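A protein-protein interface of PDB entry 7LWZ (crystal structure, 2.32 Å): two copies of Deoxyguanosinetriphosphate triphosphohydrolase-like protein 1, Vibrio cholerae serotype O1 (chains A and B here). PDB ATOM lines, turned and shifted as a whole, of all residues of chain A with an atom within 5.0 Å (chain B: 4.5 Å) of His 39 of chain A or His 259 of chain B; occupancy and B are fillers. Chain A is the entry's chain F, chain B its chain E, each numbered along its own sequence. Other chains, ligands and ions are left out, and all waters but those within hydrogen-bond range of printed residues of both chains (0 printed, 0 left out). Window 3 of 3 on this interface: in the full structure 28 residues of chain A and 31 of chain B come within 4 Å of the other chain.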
ATOM      1  N   ALA A  35      27.474  24.459   3.529  1.00  0.00           N
ATOM      2  CA  ALA A  35      27.042  24.209   2.166  1.00  0.00           C
ATOM      3  C   ALA A  35      27.813  23.044   1.545  1.00  0.00           C
ATOM      4  O   ALA A  35      27.210  22.174   0.899  1.00  0.00           O
ATOM      5  CB  ALA A  35      27.191  25.479   1.329  1.00  0.00           C
ATOM      6  N   ARG A  36      29.138  22.984   1.762  1.00  0.00           N
ATOM      7  CA  ARG A  36      29.936  21.914   1.155  1.00  0.00           C
ATOM      8  C   ARG A  36      29.517  20.558   1.674  1.00  0.00           C
ATOM      9  O   ARG A  36      29.356  19.609   0.896  1.00  0.00           O
ATOM     10  CB  ARG A  36      31.425  22.115   1.406  1.00  0.00           C
ATOM     11  CG  ARG A  36      32.025  23.213   0.564  1.00  0.00           C
ATOM     12  CD  ARG A  36      33.296  23.744   1.137  1.00  0.00           C
ATOM     13  NE  ARG A  36      33.681  24.958   0.426  1.00  0.00           N
ATOM     14  CZ  ARG A  36      34.935  25.340   0.211  1.00  0.00           C
ATOM     15  NH1 ARG A  36      35.182  26.458  -0.454  1.00  0.00           N
ATOM     16  NH2 ARG A  36      35.943  24.597   0.644  1.00  0.00           N
ATOM     17  N   ILE A  37      29.306  20.451   2.987  1.00  0.00           N
ATOM     18  CA  ILE A  37      28.922  19.166   3.555  1.00  0.00           C
ATOM     19  C   ILE A  37      27.576  18.709   2.994  1.00  0.00           C
ATOM     20  O   ILE A  37      27.431  17.563   2.546  1.00  0.00           O
ATOM     21  CB  ILE A  37      28.909  19.269   5.088  1.00  0.00           C
ATOM     22  CG1 ILE A  37      30.353  19.360   5.599  1.00  0.00           C
ATOM     23  CG2 ILE A  37      28.190  18.081   5.679  1.00  0.00           C
ATOM     24  CD1 ILE A  37      30.504  19.920   6.993  1.00  0.00           C
ATOM     25  N   LEU A  38      26.596  19.618   2.932  1.00  0.00           N
ATOM     26  CA  LEU A  38      25.278  19.259   2.408  1.00  0.00           C
ATOM     27  C   LEU A  38      25.348  18.811   0.949  1.00  0.00           C
ATOM     28  O   LEU A  38      24.594  17.921   0.535  1.00  0.00           O
ATOM     29  CB  LEU A  38      24.323  20.442   2.545  1.00  0.00           C
ATOM     30  CG  LEU A  38      23.830  20.736   3.963  1.00  0.00           C
ATOM     31  CD1 LEU A  38      23.207  22.120   4.002  1.00  0.00           C
ATOM     32  CD2 LEU A  38      22.817  19.690   4.449  1.00  0.00           C
ATOM     33  N   HIS A  39      26.267  19.373   0.170  1.00  0.00           N
ATOM     34  CA  HIS A  39      26.392  19.019  -1.233  1.00  0.00           C
ATOM     35  C   HIS A  39      27.248  17.770  -1.457  1.00  0.00           C
ATOM     36  O   HIS A  39      27.343  17.297  -2.592  1.00  0.00           O
ATOM     37  CB  HIS A  39      26.995  20.198  -2.017  1.00  0.00           C
ATOM     38  CG  HIS A  39      25.998  21.240  -2.434  1.00  0.00           C
ATOM     39  ND1 HIS A  39      25.476  21.304  -3.710  1.00  0.00           N
ATOM     40  CD2 HIS A  39      25.454  22.280  -1.755  1.00  0.00           C
ATOM     41  CE1 HIS A  39      24.641  22.327  -3.794  1.00  0.00           C
ATOM     42  NE2 HIS A  39      24.606  22.933  -2.621  1.00  0.00           N
ATOM     43  N   SER A  40      27.866  17.230  -0.412  1.00  0.00           N
ATOM     44  CA  SER A  40      28.817  16.135  -0.557  1.00  0.00           C
ATOM     45  C   SER A  40      28.143  14.777  -0.786  1.00  0.00           C
ATOM     46  O   SER A  40      27.038  14.503  -0.303  1.00  0.00           O
ATOM     47  CB  SER A  40      29.716  16.080   0.676  1.00  0.00           C
ATOM     48  OG  SER A  40      28.965  15.749   1.826  1.00  0.00           O
ATOM     49  N   ALA A  41      28.842  13.908  -1.513  1.00  0.00           N
ATOM     50  CA  ALA A  41      28.363  12.533  -1.653  1.00  0.00           C
ATOM     51  C   ALA A  41      28.344  11.820  -0.305  1.00  0.00           C
ATOM     52  O   ALA A  41      27.398  11.086   0.008  1.00  0.00           O
ATOM     53  CB  ALA A  41      29.245  11.766  -2.634  1.00  0.00           C
ATOM     54  N   ARG A  44      25.127  12.691   1.359  1.00  0.00           N
ATOM     55  CA  ARG A  44      23.943  12.109   0.724  1.00  0.00           C
ATOM     56  C   ARG A  44      23.818  10.617   1.019  1.00  0.00           C
ATOM     57  O   ARG A  44      22.698  10.098   1.092  1.00  0.00           O
ATOM     58  CB  ARG A  44      23.947  12.365  -0.786  1.00  0.00           C
ATOM     59  CG  ARG A  44      23.633  13.829  -1.170  1.00  0.00           C
ATOM     60  CD  ARG A  44      23.187  13.933  -2.629  1.00  0.00           C
ATOM     61  NE  ARG A  44      24.225  13.440  -3.539  1.00  0.00           N
ATOM     62  CZ  ARG A  44      25.239  14.173  -3.987  1.00  0.00           C
ATOM     63  NH1 ARG A  44      25.351  15.446  -3.621  1.00  0.00           N
ATOM     64  NH2 ARG A  44      26.142  13.632  -4.791  1.00  0.00           N
ATOM     65  N   ARG B  62      20.829  10.640  -5.127  1.00  0.00           N
ATOM     66  CA  ARG B  62      20.099  11.920  -5.287  1.00  0.00           C
ATOM     67  C   ARG B  62      18.607  11.610  -5.175  1.00  0.00           C
ATOM     68  O   ARG B  62      18.075  10.902  -6.040  1.00  0.00           O
ATOM     69  CB  ARG B  62      20.489  12.613  -6.595  1.00  0.00           C
ATOM     70  CG  ARG B  62      21.967  12.964  -6.674  1.00  0.00           C
ATOM     71  CD  ARG B  62      22.273  14.267  -7.385  1.00  0.00           C
ATOM     72  NE  ARG B  62      23.652  14.661  -7.152  1.00  0.00           N
ATOM     73  CZ  ARG B  62      24.060  15.911  -6.992  1.00  0.00           C
ATOM     74  NH1 ARG B  62      23.191  16.904  -7.044  1.00  0.00           N
ATOM     75  NH2 ARG B  62      25.338  16.165  -6.780  1.00  0.00           N
ATOM     76  N   GLU B  70      19.008  21.384  -2.052  1.00  0.00           N
ATOM     77  CA  GLU B  70      19.649  22.230  -3.046  1.00  0.00           C
ATOM     78  C   GLU B  70      18.775  23.434  -3.377  1.00  0.00           C
ATOM     79  O   GLU B  70      19.267  24.564  -3.480  1.00  0.00           O
ATOM     80  CB  GLU B  70      19.995  21.400  -4.290  1.00  0.00           C
ATOM     81  CG  GLU B  70      21.316  20.642  -4.086  1.00  0.00           C
ATOM     82  CD  GLU B  70      21.473  19.361  -4.909  1.00  0.00           C
ATOM     83  OE1 GLU B  70      20.590  19.033  -5.739  1.00  0.00           O
ATOM     84  OE2 GLU B  70      22.496  18.667  -4.692  1.00  0.00           O
ATOM     85  N   GLN B  73      19.181  26.134  -0.679  1.00  0.00           N
ATOM     86  CA  GLN B  73      20.392  26.950  -0.673  1.00  0.00           C
ATOM     87  C   GLN B  73      20.421  27.930  -1.844  1.00  0.00           C
ATOM     88  O   GLN B  73      20.972  29.038  -1.721  1.00  0.00           O
ATOM     89  CB  GLN B  73      21.639  26.090  -0.679  1.00  0.00           C
ATOM     90  CG  GLN B  73      21.691  25.043   0.401  1.00  0.00           C
ATOM     91  CD  GLN B  73      23.079  25.000   1.011  1.00  0.00           C
ATOM     92  OE1 GLN B  73      24.082  24.987   0.292  1.00  0.00           O
ATOM     93  NE2 GLN B  73      23.147  25.013   2.339  1.00  0.00           N
ATOM     94  N   ILE B  74      19.840  27.553  -2.991  1.00  0.00           N
ATOM     95  CA  ILE B  74      19.696  28.511  -4.080  1.00  0.00           C
ATOM     96  C   ILE B  74      18.698  29.596  -3.694  1.00  0.00           C
ATOM     97  O   ILE B  74      18.891  30.780  -4.004  1.00  0.00           O
ATOM     98  CB  ILE B  74      19.291  27.750  -5.352  1.00  0.00           C
ATOM     99  CG1 ILE B  74      20.491  26.994  -5.929  1.00  0.00           C
ATOM    100  CG2 ILE B  74      18.694  28.667  -6.372  1.00  0.00           C
ATOM    101  CD1 ILE B  74      20.107  25.855  -6.836  1.00  0.00           C
ATOM    102  N   ALA B 255      17.398  24.473  -9.436  1.00  0.00           N
ATOM    103  CA  ALA B 255      17.889  23.201  -8.909  1.00  0.00           C
ATOM    104  C   ALA B 255      17.616  22.043  -9.863  1.00  0.00           C
ATOM    105  O   ALA B 255      18.474  21.177 -10.058  1.00  0.00           O
ATOM    106  CB  ALA B 255      17.268  22.914  -7.543  1.00  0.00           C
ATOM    107  N   TYR B 256      16.400  21.977 -10.415  1.00  0.00           N
ATOM    108  CA  TYR B 256      16.057  20.931 -11.379  1.00  0.00           C
ATOM    109  C   TYR B 256      16.944  21.002 -12.620  1.00  0.00           C
ATOM    110  O   TYR B 256      17.462  19.980 -13.089  1.00  0.00           O
ATOM    111  CB  TYR B 256      14.572  21.057 -11.741  1.00  0.00           C
ATOM    112  CG  TYR B 256      14.055  20.121 -12.821  1.00  0.00           C
ATOM    113  CD1 TYR B 256      13.710  18.803 -12.529  1.00  0.00           C
ATOM    114  CD2 TYR B 256      13.877  20.572 -14.132  1.00  0.00           C
ATOM    115  CE1 TYR B 256      13.222  17.954 -13.518  1.00  0.00           C
ATOM    116  CE2 TYR B 256      13.390  19.735 -15.124  1.00  0.00           C
ATOM    117  CZ  TYR B 256      13.065  18.428 -14.812  1.00  0.00           C
ATOM    118  OH  TYR B 256      12.579  17.593 -15.793  1.00  0.00           O
ATOM    119  N   GLY B 257      17.169  22.210 -13.131  1.00  0.00           N
ATOM    120  CA  GLY B 257      17.857  22.362 -14.398  1.00  0.00           C
ATOM    121  C   GLY B 257      19.312  21.935 -14.371  1.00  0.00           C
ATOM    122  O   GLY B 257      19.819  21.417 -15.363  1.00  0.00           O
ATOM    123  N   VAL B 258      20.023  22.202 -13.275  1.00  0.00           N
ATOM    124  CA  VAL B 258      21.473  22.046 -13.241  1.00  0.00           C
ATOM    125  C   VAL B 258      21.896  20.838 -12.419  1.00  0.00           C
ATOM    126  O   VAL B 258      22.896  20.194 -12.742  1.00  0.00           O
ATOM    127  CB  VAL B 258      22.193  23.316 -12.737  1.00  0.00           C
ATOM    128  CG1 VAL B 258      21.628  24.556 -13.376  1.00  0.00           C
ATOM    129  CG2 VAL B 258      22.112  23.385 -11.241  1.00  0.00           C
ATOM    130  N   HIS B 259      21.203  20.543 -11.324  1.00  0.00           N
ATOM    131  CA  HIS B 259      21.720  19.506 -10.448  1.00  0.00           C
ATOM    132  C   HIS B 259      21.346  18.108 -10.920  1.00  0.00           C
ATOM    133  O   HIS B 259      22.029  17.145 -10.557  1.00  0.00           O
ATOM    134  CB  HIS B 259      21.251  19.743  -9.009  1.00  0.00           C
ATOM    135  CG  HIS B 259      22.144  20.663  -8.236  1.00  0.00           C
ATOM    136  ND1 HIS B 259      21.661  21.689  -7.452  1.00  0.00           N
ATOM    137  CD2 HIS B 259      23.493  20.719  -8.139  1.00  0.00           C
ATOM    138  CE1 HIS B 259      22.674  22.334  -6.902  1.00  0.00           C
ATOM    139  NE2 HIS B 259      23.797  21.767  -7.304  1.00  0.00           N
ATOM    140  N   ASP B 260      20.306  17.981 -11.745  1.00  0.00           N
ATOM    141  CA  ASP B 260      20.046  16.724 -12.430  1.00  0.00           C
ATOM    142  C   ASP B 260      21.049  16.500 -13.555  1.00  0.00           C
ATOM    143  O   ASP B 260      21.372  15.352 -13.881  1.00  0.00           O
ATOM    144  CB  ASP B 260      18.607  16.724 -12.957  1.00  0.00           C
ATOM    145  CG  ASP B 260      17.562  16.906 -11.835  1.00  0.00           C
ATOM    146  OD1 ASP B 260      17.958  17.075 -10.658  1.00  0.00           O
ATOM    147  OD2 ASP B 260      16.348  16.884 -12.128  1.00  0.00           O
ATOM    148  N   LEU B 261      21.592  17.589 -14.093  1.00  0.00           N
ATOM    149  CA  LEU B 261      22.455  17.524 -15.262  1.00  0.00           C
ATOM    150  C   LEU B 261      23.797  16.864 -14.970  1.00  0.00           C
ATOM    151  O   LEU B 261      24.335  16.159 -15.827  1.00  0.00           O
ATOM    152  CB  LEU B 261      22.652  18.932 -15.807  1.00  0.00           C
ATOM    153  CG  LEU B 261      23.672  19.173 -16.900  1.00  0.00           C
ATOM    154  CD1 LEU B 261      23.223  18.511 -18.192  1.00  0.00           C
ATOM    155  CD2 LEU B 261      23.837  20.673 -17.093  1.00  0.00           C
ATOM    156  N   GLU B 262      24.365  17.075 -13.784  1.00  0.00           N
ATOM    157  CA  GLU B 262      25.743  16.634 -13.577  1.00  0.00           C
ATOM    158  C   GLU B 262      25.861  15.103 -13.559  1.00  0.00           C
ATOM    159  O   GLU B 262      26.737  14.534 -14.215  1.00  0.00           O
ATOM    160  CB  GLU B 262      26.315  17.218 -12.292  1.00  0.00           C
ATOM    161  CG  GLU B 262      27.812  16.966 -12.214  1.00  0.00           C
ATOM    162  CD  GLU B 262      28.333  16.850 -10.799  1.00  0.00           C
ATOM    163  OE1 GLU B 262      29.503  16.422 -10.641  1.00  0.00           O
ATOM    164  OE2 GLU B 262      27.585  17.198  -9.855  1.00  0.00           O
ATOM    165  N   ASP B 263      24.992  14.401 -12.816  1.00  0.00           N
ATOM    166  CA  ASP B 263      25.147  12.939 -12.696  1.00  0.00           C
ATOM    167  C   ASP B 263      24.721  12.222 -13.969  1.00  0.00           C
ATOM    168  O   ASP B 263      25.121  11.069 -14.202  1.00  0.00           O
ATOM    169  CB  ASP B 263      24.341  12.368 -11.527  1.00  0.00           C
ATOM    170  CG  ASP B 263      24.617  13.062 -10.188  1.00  0.00           C
ATOM    171  OD1 ASP B 263      25.105  12.376  -9.269  1.00  0.00           O
ATOM    172  OD2 ASP B 263      24.262  14.259 -10.026  1.00  0.00           O
ATOM    173  N   ILE B 314      29.122  23.740 -12.672  1.00  0.00           N
ATOM    174  CA  ILE B 314      27.791  23.726 -12.065  1.00  0.00           C
ATOM    175  C   ILE B 314      27.612  24.952 -11.181  1.00  0.00           C
ATOM    176  O   ILE B 314      26.570  25.618 -11.211  1.00  0.00           O
ATOM    177  CB  ILE B 314      27.576  22.422 -11.268  1.00  0.00           C
ATOM    178  CG1 ILE B 314      27.752  21.181 -12.158  1.00  0.00           C
ATOM    179  CG2 ILE B 314      26.194  22.407 -10.590  1.00  0.00           C
ATOM    180  CD1 ILE B 314      26.645  20.967 -13.147  1.00  0.00           C
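The guanidinium group of Arg 44 of chain A lies close to the guanidinium group of Arg 62 of chain B.
The backbone carbonyl oxygen of His 39 of chain A lies within hydrogen-bond range of the guanidinium group of Arg 44 of chain A (2.9 Å). NH1 of Arg 62 of chain B lies within salt-bridge range of OE2 of Glu 70 of chain B, 3.0 Å away. OE2 of Glu 262 of chain B lies within salt-bridge range of NH2 of Arg 62 of chain B (3.9 Å). NE of Arg 62 of chain B is in salt-bridge range of OD2 of Asp 263 of chain B, 3.0 Å away. ND1 of His 259 of chain B lies within hydrogen-bond range of OE1 of Glu 70 of chain B (3.3 Å).
Among the printed residues, pairs that only touch across the chains: Ala 35 of chain A with Gln 73 of chain B (3.3 Å), Leu 38 of chain A with Gln 73 of chain B (3.3 Å), His 39 of chain A with Gln 73 of chain B (3.6 Å), His 39 of chain A with His 259 of chain B (3.7 Å) and His 39 of chain A with Glu 70 of chain B (3.7 Å).
Of the printed residues of chain B, Leu 38 of chain A touches Gln 73 (3.3 Å). Of the printed residues of chain A, Arg 62 of chain B touches Arg 44 (3.2 Å). Printed residues of chain A within 4 Å of Glu 70 of chain B: His 39 (3.7 Å). Printed residues of chain A within 4 Å of Gln 73 of chain B: Ala 35, Leu 38 and His 39. Of the printed residues of chain A, His 259 of chain B touches His 39 (3.7 Å). Asp 263 of chain B touches none of the printed residues of chain A. The nearest printed residue of chain A that does not touch His 259 of chain B is Arg 44 of chain A (7.2 Å).
Hydrophobic or aromatic side chains of chain B within 4 Å of the printed part of chain A: His 259. Of the 8 printed residues of chain A, 4 touch a printed residue of chain B. Printed residues of chain A that touch a printed residue of chain B: Ala 35, Leu 38, His 39 and Arg 44. Hydrophobic or aromatic side chains of chain A that line the printed part of chain B: Ala 35, Leu 38 and His 39. Among the printed residues, 6 pairs touch across the chains.
No position is printed for both chains.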
